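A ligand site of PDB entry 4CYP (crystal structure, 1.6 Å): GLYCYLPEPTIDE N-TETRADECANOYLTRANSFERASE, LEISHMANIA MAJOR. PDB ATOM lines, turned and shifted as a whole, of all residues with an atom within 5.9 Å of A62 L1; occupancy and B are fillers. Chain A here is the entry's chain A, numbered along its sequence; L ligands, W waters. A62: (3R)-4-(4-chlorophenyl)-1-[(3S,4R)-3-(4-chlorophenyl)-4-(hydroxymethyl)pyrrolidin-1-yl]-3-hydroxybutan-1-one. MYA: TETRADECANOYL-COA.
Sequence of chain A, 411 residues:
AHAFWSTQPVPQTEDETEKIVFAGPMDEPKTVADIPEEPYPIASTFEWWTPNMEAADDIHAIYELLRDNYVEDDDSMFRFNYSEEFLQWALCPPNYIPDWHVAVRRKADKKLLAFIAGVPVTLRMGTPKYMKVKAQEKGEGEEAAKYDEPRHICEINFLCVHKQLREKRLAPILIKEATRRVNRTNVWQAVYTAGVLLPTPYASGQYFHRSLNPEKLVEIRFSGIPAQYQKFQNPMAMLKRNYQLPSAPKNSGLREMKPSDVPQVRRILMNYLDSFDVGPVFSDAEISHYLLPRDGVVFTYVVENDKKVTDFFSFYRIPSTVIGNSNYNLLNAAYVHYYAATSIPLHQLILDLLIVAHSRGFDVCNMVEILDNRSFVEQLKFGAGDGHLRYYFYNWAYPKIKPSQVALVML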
ATOM      1  N   TYR A  70      -5.795 -30.540  -4.254  1.00  0.00           N
ATOM      2  CA  TYR A  70      -6.152 -29.109  -4.161  1.00  0.00           C
ATOM      3  C   TYR A  70      -5.373 -28.250  -5.178  1.00  0.00           C
ATOM      4  O   TYR A  70      -4.836 -28.787  -6.153  1.00  0.00           O
ATOM      5  CB  TYR A  70      -6.036 -28.614  -2.763  1.00  0.00           C
ATOM      6  CG  TYR A  70      -6.855 -27.330  -2.451  1.00  0.00           C
ATOM      7  CD1 TYR A  70      -8.234 -27.202  -2.900  1.00  0.00           C
ATOM      8  CD2 TYR A  70      -6.238 -26.293  -1.663  1.00  0.00           C
ATOM      9  CE1 TYR A  70      -8.963 -26.070  -2.538  1.00  0.00           C
ATOM     10  CE2 TYR A  70      -6.937 -25.139  -1.317  1.00  0.00           C
ATOM     11  CZ  TYR A  70      -8.297 -25.043  -1.744  1.00  0.00           C
ATOM     12  OH  TYR A  70      -8.972 -23.860  -1.425  1.00  0.00           O
ATOM     13  N   VAL A  71      -5.343 -26.933  -4.994  1.00  0.00           N
ATOM     14  CA  VAL A  71      -4.869 -25.966  -6.053  1.00  0.00           C
ATOM     15  C   VAL A  71      -3.370 -26.255  -6.457  1.00  0.00           C
ATOM     16  O   VAL A  71      -2.528 -26.373  -5.591  1.00  0.00           O
ATOM     17  CB  VAL A  71      -5.034 -24.521  -5.512  1.00  0.00           C
ATOM     18  CG1 VAL A  71      -4.464 -23.464  -6.497  1.00  0.00           C
ATOM     19  CG2 VAL A  71      -6.559 -24.197  -5.224  1.00  0.00           C
ATOM     20  N   PHE A  80      -0.630 -26.839  -3.202  1.00  0.00           N
ATOM     21  CA  PHE A  80      -0.713 -26.496  -1.784  1.00  0.00           C
ATOM     22  C   PHE A  80      -0.829 -27.732  -0.871  1.00  0.00           C
ATOM     23  O   PHE A  80      -1.535 -28.734  -1.248  1.00  0.00           O
ATOM     24  CB  PHE A  80      -1.981 -25.600  -1.528  1.00  0.00           C
ATOM     25  CG  PHE A  80      -1.823 -24.201  -2.015  1.00  0.00           C
ATOM     26  CD1 PHE A  80      -2.098 -23.885  -3.389  1.00  0.00           C
ATOM     27  CD2 PHE A  80      -1.506 -23.199  -1.124  1.00  0.00           C
ATOM     28  CE1 PHE A  80      -1.967 -22.552  -3.827  1.00  0.00           C
ATOM     29  CE2 PHE A  80      -1.361 -21.886  -1.577  1.00  0.00           C
ATOM     30  CZ  PHE A  80      -1.590 -21.583  -2.912  1.00  0.00           C
ATOM     31  N   TYR A  82      -1.790 -27.585   2.888  1.00  0.00           N
ATOM     32  CA  TYR A  82      -2.255 -27.123   4.182  1.00  0.00           C
ATOM     33  C   TYR A  82      -2.103 -28.200   5.266  1.00  0.00           C
ATOM     34  O   TYR A  82      -2.534 -29.384   5.004  1.00  0.00           O
ATOM     35  CB  TYR A  82      -3.743 -26.747   4.040  1.00  0.00           C
ATOM     36  CG  TYR A  82      -4.041 -25.488   3.258  1.00  0.00           C
ATOM     37  CD1 TYR A  82      -4.213 -25.537   1.862  1.00  0.00           C
ATOM     38  CD2 TYR A  82      -4.188 -24.254   3.914  1.00  0.00           C
ATOM     39  CE1 TYR A  82      -4.553 -24.378   1.107  1.00  0.00           C
ATOM     40  CE2 TYR A  82      -4.533 -23.107   3.140  1.00  0.00           C
ATOM     41  CZ  TYR A  82      -4.667 -23.174   1.794  1.00  0.00           C
ATOM     42  OH  TYR A  82      -4.997 -21.976   1.205  1.00  0.00           O
ATOM     43  N   PHE A  86      -3.223 -26.295  10.666  1.00  0.00           N
ATOM     44  CA  PHE A  86      -3.809 -25.170   9.871  1.00  0.00           C
ATOM     45  C   PHE A  86      -5.316 -25.325   9.569  1.00  0.00           C
ATOM     46  O   PHE A  86      -6.136 -24.403   9.744  1.00  0.00           O
ATOM     47  CB  PHE A  86      -3.016 -24.961   8.595  1.00  0.00           C
ATOM     48  CG  PHE A  86      -3.304 -23.639   7.879  1.00  0.00           C
ATOM     49  CD1 PHE A  86      -4.536 -23.426   7.239  1.00  0.00           C
ATOM     50  CD2 PHE A  86      -2.294 -22.607   7.851  1.00  0.00           C
ATOM     51  CE1 PHE A  86      -4.806 -22.197   6.614  1.00  0.00           C
ATOM     52  CE2 PHE A  86      -2.535 -21.400   7.130  1.00  0.00           C
ATOM     53  CZ  PHE A  86      -3.733 -21.176   6.510  1.00  0.00           C
ATOM     54  N   ILE A 156     -16.722 -18.912   2.110  1.00  0.00           N
ATOM     55  CA  ILE A 156     -16.498 -20.222   1.513  1.00  0.00           C
ATOM     56  C   ILE A 156     -15.022 -20.391   1.188  1.00  0.00           C
ATOM     57  O   ILE A 156     -14.348 -19.416   0.819  1.00  0.00           O
ATOM     58  CB  ILE A 156     -17.358 -20.398   0.230  1.00  0.00           C
ATOM     59  CG1 ILE A 156     -18.866 -20.456   0.681  1.00  0.00           C
ATOM     60  CG2 ILE A 156     -16.970 -21.669  -0.533  1.00  0.00           C
ATOM     61  CD1 ILE A 156     -19.341 -21.834   1.150  1.00  0.00           C
ATOM     62  N   ASN A 157     -14.533 -21.640   1.375  1.00  0.00           N
ATOM     63  CA  ASN A 157     -13.072 -21.888   1.030  1.00  0.00           C
ATOM     64  C   ASN A 157     -12.974 -23.396   0.847  1.00  0.00           C
ATOM     65  O   ASN A 157     -13.913 -24.159   1.083  1.00  0.00           O
ATOM     66  CB  ASN A 157     -12.200 -21.395   2.212  1.00  0.00           C
ATOM     67  CG  ASN A 157     -10.737 -21.078   1.808  1.00  0.00           C
ATOM     68  OD1 ASN A 157     -10.285 -21.468   0.711  1.00  0.00           O
ATOM     69  ND2 ASN A 157     -10.054 -20.340   2.624  1.00  0.00           N
ATOM     70  N   PHE A 158     -11.833 -23.868   0.324  1.00  0.00           N
ATOM     71  CA  PHE A 158     -11.509 -25.282   0.286  1.00  0.00           C
ATOM     72  C   PHE A 158     -12.403 -26.128  -0.587  1.00  0.00           C
ATOM     73  O   PHE A 158     -12.538 -27.337  -0.310  1.00  0.00           O
ATOM     74  CB  PHE A 158     -11.295 -25.859   1.689  1.00  0.00           C
ATOM     75  CG  PHE A 158     -10.272 -25.154   2.508  1.00  0.00           C
ATOM     76  CD1 PHE A 158      -8.876 -25.242   2.143  1.00  0.00           C
ATOM     77  CD2 PHE A 158     -10.627 -24.402   3.601  1.00  0.00           C
ATOM     78  CE1 PHE A 158      -7.918 -24.522   2.974  1.00  0.00           C
ATOM     79  CE2 PHE A 158      -9.703 -23.710   4.406  1.00  0.00           C
ATOM     80  CZ  PHE A 158      -8.329 -23.769   4.062  1.00  0.00           C
ATOM     81  N   THR A 193     -13.304 -16.336  -2.971  1.00  0.00           N
ATOM     82  CA  THR A 193     -12.299 -15.847  -3.948  1.00  0.00           C
ATOM     83  C   THR A 193     -11.929 -17.093  -4.834  1.00  0.00           C
ATOM     84  O   THR A 193     -12.139 -18.245  -4.475  1.00  0.00           O
ATOM     85  CB  THR A 193     -11.064 -15.324  -3.208  1.00  0.00           C
ATOM     86  OG1 THR A 193     -10.589 -16.314  -2.220  1.00  0.00           O
ATOM     87  CG2 THR A 193     -11.282 -13.934  -2.561  1.00  0.00           C
ATOM     88  N   ALA A 194     -11.383 -16.828  -6.019  1.00  0.00           N
ATOM     89  CA  ALA A 194     -10.823 -17.871  -6.878  1.00  0.00           C
ATOM     90  C   ALA A 194      -9.711 -17.266  -7.735  1.00  0.00           C
ATOM     91  O   ALA A 194      -9.697 -16.042  -8.088  1.00  0.00           O
ATOM     92  CB  ALA A 194     -11.883 -18.545  -7.750  1.00  0.00           C
ATOM     93  N   GLY A 195      -8.755 -18.145  -8.070  1.00  0.00           N
ATOM     94  CA  GLY A 195      -7.718 -17.754  -9.048  1.00  0.00           C
ATOM     95  C   GLY A 195      -8.222 -18.029 -10.476  1.00  0.00           C
ATOM     96  O   GLY A 195      -7.385 -18.034 -11.437  1.00  0.00           O
ATOM     97  N   TYR A 207      -1.031 -11.171  -7.708  1.00  0.00           N
ATOM     98  CA  TYR A 207      -0.259 -11.840  -6.645  1.00  0.00           C
ATOM     99  C   TYR A 207       1.120 -11.228  -6.598  1.00  0.00           C
ATOM    100  O   TYR A 207       1.669 -10.823  -7.678  1.00  0.00           O
ATOM    101  CB  TYR A 207      -0.130 -13.285  -7.011  1.00  0.00           C
ATOM    102  CG  TYR A 207      -1.420 -14.036  -7.168  1.00  0.00           C
ATOM    103  CD1 TYR A 207      -2.102 -14.444  -6.024  1.00  0.00           C
ATOM    104  CD2 TYR A 207      -1.899 -14.442  -8.431  1.00  0.00           C
ATOM    105  CE1 TYR A 207      -3.235 -15.224  -6.120  1.00  0.00           C
ATOM    106  CE2 TYR A 207      -3.053 -15.231  -8.536  1.00  0.00           C
ATOM    107  CZ  TYR A 207      -3.715 -15.592  -7.352  1.00  0.00           C
ATOM    108  OH  TYR A 207      -4.834 -16.424  -7.473  1.00  0.00           O
ATOM    109  N   PHE A 208       1.763 -11.225  -5.426  1.00  0.00           N
ATOM    110  CA  PHE A 208       3.154 -10.729  -5.293  1.00  0.00           C
ATOM    111  C   PHE A 208       4.011 -11.662  -4.440  1.00  0.00           C
ATOM    112  O   PHE A 208       3.472 -12.274  -3.571  1.00  0.00           O
ATOM    113  CB  PHE A 208       3.205  -9.308  -4.636  1.00  0.00           C
ATOM    114  CG  PHE A 208       2.721  -8.234  -5.565  1.00  0.00           C
ATOM    115  CD1 PHE A 208       1.377  -7.954  -5.680  1.00  0.00           C
ATOM    116  CD2 PHE A 208       3.667  -7.566  -6.442  1.00  0.00           C
ATOM    117  CE1 PHE A 208       0.902  -7.061  -6.619  1.00  0.00           C
ATOM    118  CE2 PHE A 208       3.182  -6.656  -7.428  1.00  0.00           C
ATOM    119  CZ  PHE A 208       1.796  -6.406  -7.474  1.00  0.00           C
ATOM    120  N   HIS A 209       5.318 -11.777  -4.762  1.00  0.00           N
ATOM    121  CA  HIS A 209       6.279 -12.720  -4.056  1.00  0.00           C
ATOM    122  C   HIS A 209       7.544 -11.985  -3.677  1.00  0.00           C
ATOM    123  O   HIS A 209       7.978 -11.147  -4.473  1.00  0.00           O
ATOM    124  CB  HIS A 209       6.745 -13.911  -4.962  1.00  0.00           C
ATOM    125  CG  HIS A 209       5.634 -14.561  -5.709  1.00  0.00           C
ATOM    126  ND1 HIS A 209       4.689 -15.355  -5.067  1.00  0.00           N
ATOM    127  CD2 HIS A 209       5.272 -14.527  -7.007  1.00  0.00           C
ATOM    128  CE1 HIS A 209       3.836 -15.840  -5.958  1.00  0.00           C
ATOM    129  NE2 HIS A 209       4.134 -15.325  -7.139  1.00  0.00           N
ATOM    130  N   TYR A 316       0.963 -16.113   7.960  1.00  0.00           N
ATOM    131  CA  TYR A 316       0.638 -17.540   8.130  1.00  0.00           C
ATOM    132  C   TYR A 316       1.427 -18.423   7.231  1.00  0.00           C
ATOM    133  O   TYR A 316       1.936 -18.010   6.199  1.00  0.00           O
ATOM    134  CB  TYR A 316      -0.911 -17.752   8.060  1.00  0.00           C
ATOM    135  CG  TYR A 316      -1.512 -17.315   6.732  1.00  0.00           C
ATOM    136  CD1 TYR A 316      -1.558 -18.181   5.623  1.00  0.00           C
ATOM    137  CD2 TYR A 316      -2.103 -16.062   6.672  1.00  0.00           C
ATOM    138  CE1 TYR A 316      -2.126 -17.808   4.389  1.00  0.00           C
ATOM    139  CE2 TYR A 316      -2.629 -15.641   5.459  1.00  0.00           C
ATOM    140  CZ  TYR A 316      -2.676 -16.488   4.365  1.00  0.00           C
ATOM    141  OH  TYR A 316      -3.202 -16.048   3.167  1.00  0.00           O
ATOM    142  N   ILE A 318       1.904 -21.800   4.756  1.00  0.00           N
ATOM    143  CA  ILE A 318       1.365 -22.931   4.012  1.00  0.00           C
ATOM    144  C   ILE A 318       2.508 -23.454   3.181  1.00  0.00           C
ATOM    145  O   ILE A 318       3.002 -22.732   2.298  1.00  0.00           O
ATOM    146  CB  ILE A 318       0.216 -22.582   3.015  1.00  0.00           C
ATOM    147  CG1 ILE A 318      -0.899 -21.751   3.718  1.00  0.00           C
ATOM    148  CG2 ILE A 318      -0.409 -23.928   2.535  1.00  0.00           C
ATOM    149  CD1 ILE A 318      -1.800 -21.102   2.662  1.00  0.00           C
ATOM    150  N   TYR A 335       2.766 -16.049   4.230  1.00  0.00           N
ATOM    151  CA  TYR A 335       1.716 -15.217   3.529  1.00  0.00           C
ATOM    152  C   TYR A 335       1.375 -14.074   4.447  1.00  0.00           C
ATOM    153  O   TYR A 335       1.124 -14.230   5.632  1.00  0.00           O
ATOM    154  CB  TYR A 335       0.419 -16.046   3.331  1.00  0.00           C
ATOM    155  CG  TYR A 335       0.641 -17.102   2.254  1.00  0.00           C
ATOM    156  CD1 TYR A 335       1.289 -18.334   2.584  1.00  0.00           C
ATOM    157  CD2 TYR A 335       0.178 -16.908   0.955  1.00  0.00           C
ATOM    158  CE1 TYR A 335       1.514 -19.312   1.599  1.00  0.00           C
ATOM    159  CE2 TYR A 335       0.435 -17.871  -0.073  1.00  0.00           C
ATOM    160  CZ  TYR A 335       1.122 -19.058   0.319  1.00  0.00           C
ATOM    161  OH  TYR A 335       1.369 -20.049  -0.681  1.00  0.00           O
ATOM    162  N   ASN A 366       4.571 -14.282   0.406  1.00  0.00           N
ATOM    163  CA  ASN A 366       3.550 -14.025  -0.629  1.00  0.00           C
ATOM    164  C   ASN A 366       2.347 -13.171  -0.148  1.00  0.00           C
ATOM    165  O   ASN A 366       2.088 -13.114   1.059  1.00  0.00           O
ATOM    166  CB  ASN A 366       2.909 -15.390  -1.000  1.00  0.00           C
ATOM    167  CG  ASN A 366       3.845 -16.312  -1.720  1.00  0.00           C
ATOM    168  OD1 ASN A 366       4.704 -15.856  -2.406  1.00  0.00           O
ATOM    169  ND2 ASN A 366       3.600 -17.666  -1.638  1.00  0.00           N
ATOM    170  N   MET A 367       1.681 -12.459  -1.090  1.00  0.00           N
ATOM    171  CA  MET A 367       0.556 -11.619  -0.693  1.00  0.00           C
ATOM    172  C   MET A 367      -0.213 -11.246  -1.993  1.00  0.00           C
ATOM    173  O   MET A 367       0.264 -11.397  -3.126  1.00  0.00           O
ATOM    174  CB  MET A 367       1.097 -10.318   0.002  1.00  0.00           C
ATOM    175  CG  MET A 367       1.789  -9.295  -0.922  1.00  0.00           C
ATOM    176  SD  MET A 367       2.352  -7.914  -0.019  1.00  0.00           S
ATOM    177  CE  MET A 367       3.158  -6.949  -1.408  1.00  0.00           C
ATOM    178  N   VAL A 368      -1.442 -10.804  -1.802  1.00  0.00           N
ATOM    179  CA  VAL A 368      -2.244 -10.209  -2.949  1.00  0.00           C
ATOM    180  C   VAL A 368      -2.218  -8.678  -2.712  1.00  0.00           C
ATOM    181  O   VAL A 368      -1.966  -8.199  -1.601  1.00  0.00           O
ATOM    182  CB  VAL A 368      -3.673 -10.726  -2.954  1.00  0.00           C
ATOM    183  CG1 VAL A 368      -4.472 -10.063  -4.121  1.00  0.00           C
ATOM    184  CG2 VAL A 368      -3.640 -12.233  -3.121  1.00  0.00           C
ATOM    185  N   LEU A 389      -5.985 -12.858  -8.419  1.00  0.00           N
ATOM    186  CA  LEU A 389      -7.027 -13.365  -7.513  1.00  0.00           C
ATOM    187  C   LEU A 389      -8.319 -12.531  -7.690  1.00  0.00           C
ATOM    188  O   LEU A 389      -8.227 -11.307  -7.692  1.00  0.00           O
ATOM    189  CB  LEU A 389      -6.525 -13.314  -6.072  1.00  0.00           C
ATOM    190  CG  LEU A 389      -7.460 -13.997  -5.065  1.00  0.00           C
ATOM    191  CD1 LEU A 389      -7.515 -15.509  -5.290  1.00  0.00           C
ATOM    192  CD2 LEU A 389      -7.062 -13.646  -3.625  1.00  0.00           C
ATOM    193  N   MET A 410      -8.034 -13.979   2.609  1.00  0.00           N
ATOM    194  CA  MET A 410      -8.622 -15.277   2.484  1.00  0.00           C
ATOM    195  C   MET A 410      -7.523 -16.366   2.658  1.00  0.00           C
ATOM    196  O   MET A 410      -6.533 -16.411   1.896  1.00  0.00           O
ATOM    197  CB  MET A 410      -9.250 -15.536   1.115  1.00  0.00           C
ATOM    198  CG  MET A 410     -10.409 -14.604   0.742  1.00  0.00           C
ATOM    199  SD  MET A 410     -11.847 -15.022   1.751  1.00  0.00           S
ATOM    200  CE  MET A 410     -12.042 -16.782   1.401  1.00  0.00           C
ATOM    201  N   LEU A 411      -7.717 -17.225   3.633  1.00  0.00           N
ATOM    202  CA  LEU A 411      -6.636 -18.159   4.012  1.00  0.00           C
ATOM    203  C   LEU A 411      -6.476 -19.291   2.963  1.00  0.00           C
ATOM    204  O   LEU A 411      -7.419 -19.747   2.234  1.00  0.00           O
ATOM    205  CB  LEU A 411      -6.982 -18.827   5.369  1.00  0.00           C
ATOM    206  CG  LEU A 411      -7.003 -17.870   6.552  1.00  0.00           C
ATOM    207  CD1 LEU A 411      -7.559 -18.691   7.720  1.00  0.00           C
ATOM    208  CD2 LEU A 411      -5.683 -17.138   6.852  1.00  0.00           C
ATOM    209  OXT LEU A 411      -5.338 -19.886   2.861  1.00  0.00           O
HETATM  210  C   A62 L   1      -3.260 -18.892   0.333  1.00  0.00           C
HETATM  211  N   A62 L   1      -6.294 -17.770  -1.429  1.00  0.00           N
HETATM  212  O   A62 L   1      -3.618 -18.207   1.528  1.00  0.00           O
HETATM  213 CL   A62 L   1       0.981 -15.182  -3.911  1.00  0.00          CL
HETATM  214  C1  A62 L   1      -4.144 -18.502  -0.855  1.00  0.00           C
HETATM  215  O1  A62 L   1      -8.101 -16.801  -2.370  1.00  0.00           O
HETATM  216 CL1  A62 L   1      -3.630 -19.431  -5.819  1.00  0.00          CL
HETATM  217  C2  A62 L   1      -5.626 -18.720  -0.522  1.00  0.00           C
HETATM  218  O2  A62 L   1     -10.607 -20.064  -1.638  1.00  0.00           O
HETATM  219  C3  A62 L   1      -5.305 -16.800  -2.014  1.00  0.00           C
HETATM  220  C4  A62 L   1      -4.050 -17.015  -1.122  1.00  0.00           C
HETATM  221  C5  A62 L   1      -2.790 -16.634  -1.882  1.00  0.00           C
HETATM  222  C6  A62 L   1      -2.411 -17.360  -3.012  1.00  0.00           C
HETATM  223  C7  A62 L   1      -1.221 -16.921  -3.659  1.00  0.00           C
HETATM  224  C8  A62 L   1      -0.531 -15.807  -3.128  1.00  0.00           C
HETATM  225  C9  A62 L   1      -0.903 -15.030  -2.076  1.00  0.00           C
HETATM  226  C10 A62 L   1      -2.065 -15.500  -1.428  1.00  0.00           C
HETATM  227  C11 A62 L   1      -7.628 -17.713  -1.677  1.00  0.00           C
HETATM  228  C12 A62 L   1      -8.566 -18.763  -1.054  1.00  0.00           C
HETATM  229  C13 A62 L   1      -9.423 -19.439  -2.151  1.00  0.00           C
HETATM  230  C14 A62 L   1      -8.716 -20.649  -2.794  1.00  0.00           C
HETATM  231  C15 A62 L   1      -7.451 -20.349  -3.552  1.00  0.00           C
HETATM  232  C16 A62 L   1      -6.278 -21.002  -3.154  1.00  0.00           C
HETATM  233  C17 A62 L   1      -5.101 -20.684  -3.871  1.00  0.00           C
HETATM  234  C18 A62 L   1      -5.161 -19.788  -4.949  1.00  0.00           C
HETATM  235  C19 A62 L   1      -6.328 -19.141  -5.344  1.00  0.00           C
HETATM  236  C20 A62 L   1      -7.511 -19.468  -4.635  1.00  0.00           C
HETATM  237  S1  MYA L   2     -11.448 -21.594  -5.210  1.00  0.00           S
HETATM  238  C2  MYA L   2     -10.446 -23.145  -5.076  1.00  0.00           C
HETATM  239  C3  MYA L   2     -11.146 -24.139  -5.966  1.00  0.00           C
HETATM  240  N4  MYA L   2     -10.424 -25.409  -5.860  1.00  0.00           N
HETATM  241  C5  MYA L   2      -9.430 -25.799  -6.719  1.00  0.00           C
HETATM  242  O5  MYA L   2      -9.072 -25.111  -7.696  1.00  0.00           O
HETATM  243  C6  MYA L   2      -8.855 -27.184  -6.424  1.00  0.00           C
HETATM  244  C7  MYA L   2      -8.590 -28.039  -7.692  1.00  0.00           C
HETATM  245  N8  MYA L   2      -9.725 -28.114  -8.596  1.00  0.00           N
HETATM  246  C9  MYA L   2     -10.827 -28.824  -8.261  1.00  0.00           C
HETATM  247  O9  MYA L   2     -10.849 -29.434  -7.200  1.00  0.00           O
HETATM  248  C10 MYA L   2     -11.960 -28.878  -9.193  1.00  0.00           C
HETATM  249  O10 MYA L   2     -11.571 -28.543 -10.524  1.00  0.00           O
HETATM  250  C11 MYA L   2     -13.087 -27.884  -8.799  1.00  0.00           C
HETATM  251  C12 MYA L   2     -14.105 -27.906  -9.909  1.00  0.00           C
HETATM  252  C13 MYA L   2     -12.661 -26.443  -8.643  1.00  0.00           C
HETATM  253  C14 MYA L   2     -13.672 -28.265  -7.437  1.00  0.00           C
HETATM  254  N1A MYA L   2     -15.456 -21.882  -7.980  1.00  0.00           N
HETATM  255  O1A MYA L   2     -17.741 -30.453 -13.658  1.00  0.00           O
HETATM  256  P1A MYA L   2     -17.404 -29.741 -12.358  1.00  0.00           P
HETATM  257  C1X MYA L   2     -17.501 -24.183 -12.073  1.00  0.00           C
HETATM  258  C2A MYA L   2     -16.740 -21.940  -8.441  1.00  0.00           C
HETATM  259  O2A MYA L   2     -17.655 -30.454 -11.137  1.00  0.00           O
HETATM  260  P2A MYA L   2     -14.573 -29.871 -11.701  1.00  0.00           P
HETATM  261  C2M MYA L   2     -12.590 -21.864  -3.930  1.00  0.00           C
HETATM  262  O2M MYA L   2     -12.408 -22.742  -3.048  1.00  0.00           O
HETATM  263  C2X MYA L   2     -17.417 -24.174 -13.624  1.00  0.00           C
HETATM  264  O2X MYA L   2     -17.331 -22.831 -14.038  1.00  0.00           O
HETATM  265  N3A MYA L   2     -17.120 -22.628  -9.563  1.00  0.00           N
HETATM  266  O3A MYA L   2     -15.832 -29.240 -12.453  1.00  0.00           O
HETATM  267  C3M MYA L   2     -13.743 -20.936  -3.853  1.00  0.00           C
HETATM  268  C3X MYA L   2     -18.626 -25.024 -13.955  1.00  0.00           C
HETATM  269  O3X MYA L   2     -19.850 -24.309 -13.968  1.00  0.00           O
HETATM  270  P3X MYA L   2     -20.530 -23.709 -15.306  1.00  0.00           P
HETATM  271  C4A MYA L   2     -16.137 -23.221 -10.282  1.00  0.00           C
HETATM  272  O4A MYA L   2     -14.682 -31.337 -11.494  1.00  0.00           O
HETATM  273  C4M MYA L   2     -15.015 -21.758  -4.176  1.00  0.00           C
HETATM  274  C4X MYA L   2     -18.662 -25.992 -12.864  1.00  0.00           C
HETATM  275  O4X MYA L   2     -17.853 -25.478 -11.776  1.00  0.00           O
HETATM  276  C5A MYA L   2     -14.785 -23.188  -9.871  1.00  0.00           C
HETATM  277  O5A MYA L   2     -13.424 -29.291 -12.486  1.00  0.00           O
HETATM  278  C5M MYA L   2     -16.298 -20.891  -4.362  1.00  0.00           C
HETATM  279  C5X MYA L   2     -18.102 -27.333 -13.323  1.00  0.00           C
HETATM  280  O5X MYA L   2     -18.125 -28.303 -12.314  1.00  0.00           O
HETATM  281  C6A MYA L   2     -14.437 -22.471  -8.707  1.00  0.00           C
HETATM  282  N6A MYA L   2     -13.138 -22.381  -8.233  1.00  0.00           N
HETATM  283  O6A MYA L   2     -14.650 -29.182 -10.205  1.00  0.00           O
HETATM  284  C6M MYA L   2     -17.473 -21.814  -4.711  1.00  0.00           C
HETATM  285  N7A MYA L   2     -14.038 -23.894 -10.803  1.00  0.00           N
HETATM  286  O7A MYA L   2     -21.726 -22.815 -14.889  1.00  0.00           O
HETATM  287  C7M MYA L   2     -18.740 -20.968  -4.838  1.00  0.00           C
HETATM  288  C8A MYA L   2     -14.922 -24.336 -11.730  1.00  0.00           C
HETATM  289  O8A MYA L   2     -20.845 -24.957 -16.053  1.00  0.00           O
HETATM  290  C8M MYA L   2     -19.370 -20.709  -3.434  1.00  0.00           C
HETATM  291  N9A MYA L   2     -16.234 -23.938 -11.396  1.00  0.00           N
HETATM  292  O9A MYA L   2     -19.516 -22.722 -15.749  1.00  0.00           O
HETATM  293  C9M MYA L   2     -20.754 -19.984  -3.753  1.00  0.00           C
HETATM  294  CAM MYA L   2     -21.521 -19.638  -2.458  1.00  0.00           C
HETATM  295  CBM MYA L   2     -22.089 -20.861  -1.748  1.00  0.00           C
HETATM  296  CCM MYA L   2     -22.696 -20.503  -0.330  1.00  0.00           C
HETATM  297  CDM MYA L   2     -24.021 -19.685  -0.463  1.00  0.00           C
HETATM  298  CEM MYA L   2     -24.576 -19.297   0.940  1.00  0.00           C
HETATM  299  CFM MYA L   2     -25.645 -18.179   0.853  1.00  0.00           C
HETATM  300  O   HOH W   1     -13.005 -18.619  -1.309  1.00  0.00           O
HETATM  301  O   HOH W   2      -7.563 -22.130   0.043  1.00  0.00           O
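An oxygen (O1) of A62 L1 sits at hydrogen-bond distance from the side-chain hydroxyl (OG1) of Thr 193 (2.5 Å). OXT of Leu 411 is in hydrogen-bond range of O of A62 L1 (2.7 Å). An oxygen (O) of A62 L1 is in hydrogen-bond range of the side-chain hydroxyl (OH) of Tyr 316, at 2.7 Å. An oxygen (O2) of A62 L1 is in hydrogen-bond range of the side-chain amide oxygen (OD1) of Asn 157, 2.8 Å away. The backbone carbonyl oxygen of Met 410 is in hydrogen-bond range of an oxygen (O) of A62 L1 (3.4 Å).
The backbone carbonyl oxygen (O) of Met 367 lies within hydrogen-bond range of the backbone NH (N) of Phe 208, 2.8 Å away. OH of Tyr 70 is in hydrogen-bond range of OD1 of Asn 157 (3.5 Å). The backbone NH of Tyr 335 is in hydrogen-bond range of the backbone carbonyl oxygen of Tyr 316 (2.9 Å). The chain-end carboxylate (OXT) of Leu 411 is in hydrogen-bond range of the side-chain hydroxyl (OH) of Tyr 82 (2.7 Å). N of Phe 80 is in hydrogen-bond range of O of Val 71 (3.1 Å). The side-chain hydroxyl (OH) of Tyr 70 is in hydrogen-bond range of the backbone NH (N) of Phe 158. ND2 of Asn 157 lies within hydrogen-bond range of O of Leu 411. ND1 of His 209 lies within hydrogen-bond range of OD1 of Asn 366.
OH of Tyr 70 touches C14 of A62 L1, 3.5 Å away. CG2 of Val 71 touches C16 of A62 L1, at 3.8 Å. Phe 80 touches A62 L1 (CE1 to C17, 3.6 Å). Tyr 82 touches A62 L1. N of Gly 195 touches C19 of A62 L1 (3.8 Å). CD1 of Tyr 207 touches C7 of A62 L1 (3.5 Å). Phe 208 touches A62 L1. His 209 touches A62 L1. CD1 of Ile 318 touches C of A62 L1, at 3.5 Å. Tyr 335 touches A62 L1 (CD2 to C10, 3.6 Å). Asn 366 touches A62 L1 (CB to CL, 3.5 Å). Met 367 touches A62 L1. Leu 389 touches A62 L1. Hydrophobic or aromatic side chains within 4 Å of A62 L1: Val 71, Phe 80, Tyr 207, His 209, Tyr 316, Ile 318, Tyr 335, Leu 389 and Met 410. Within 4 Å of A62 L1: Tyr 70, Val 71, Phe 80, Tyr 82, Asn 157, Thr 193, Gly 195, Tyr 207, Phe 208, His 209, Tyr 316, Ile 318, Tyr 335, Asn 366, Met 367, Leu 389, Met 410 and Leu 411. The nearest printed residue that does not touch A62 L1 is Val 368 (4.003 Å).
Water W1 lies within hydrogen-bond range of O of Ile 156 (2.6 Å), O2 of A62 L1 (2.8 Å) and N of Thr 193 (2.8 Å). Water W2 lies within hydrogen-bond range of OH of Tyr 70, OH of Tyr 82, OD1 of Asn 157 and O of Leu 411.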
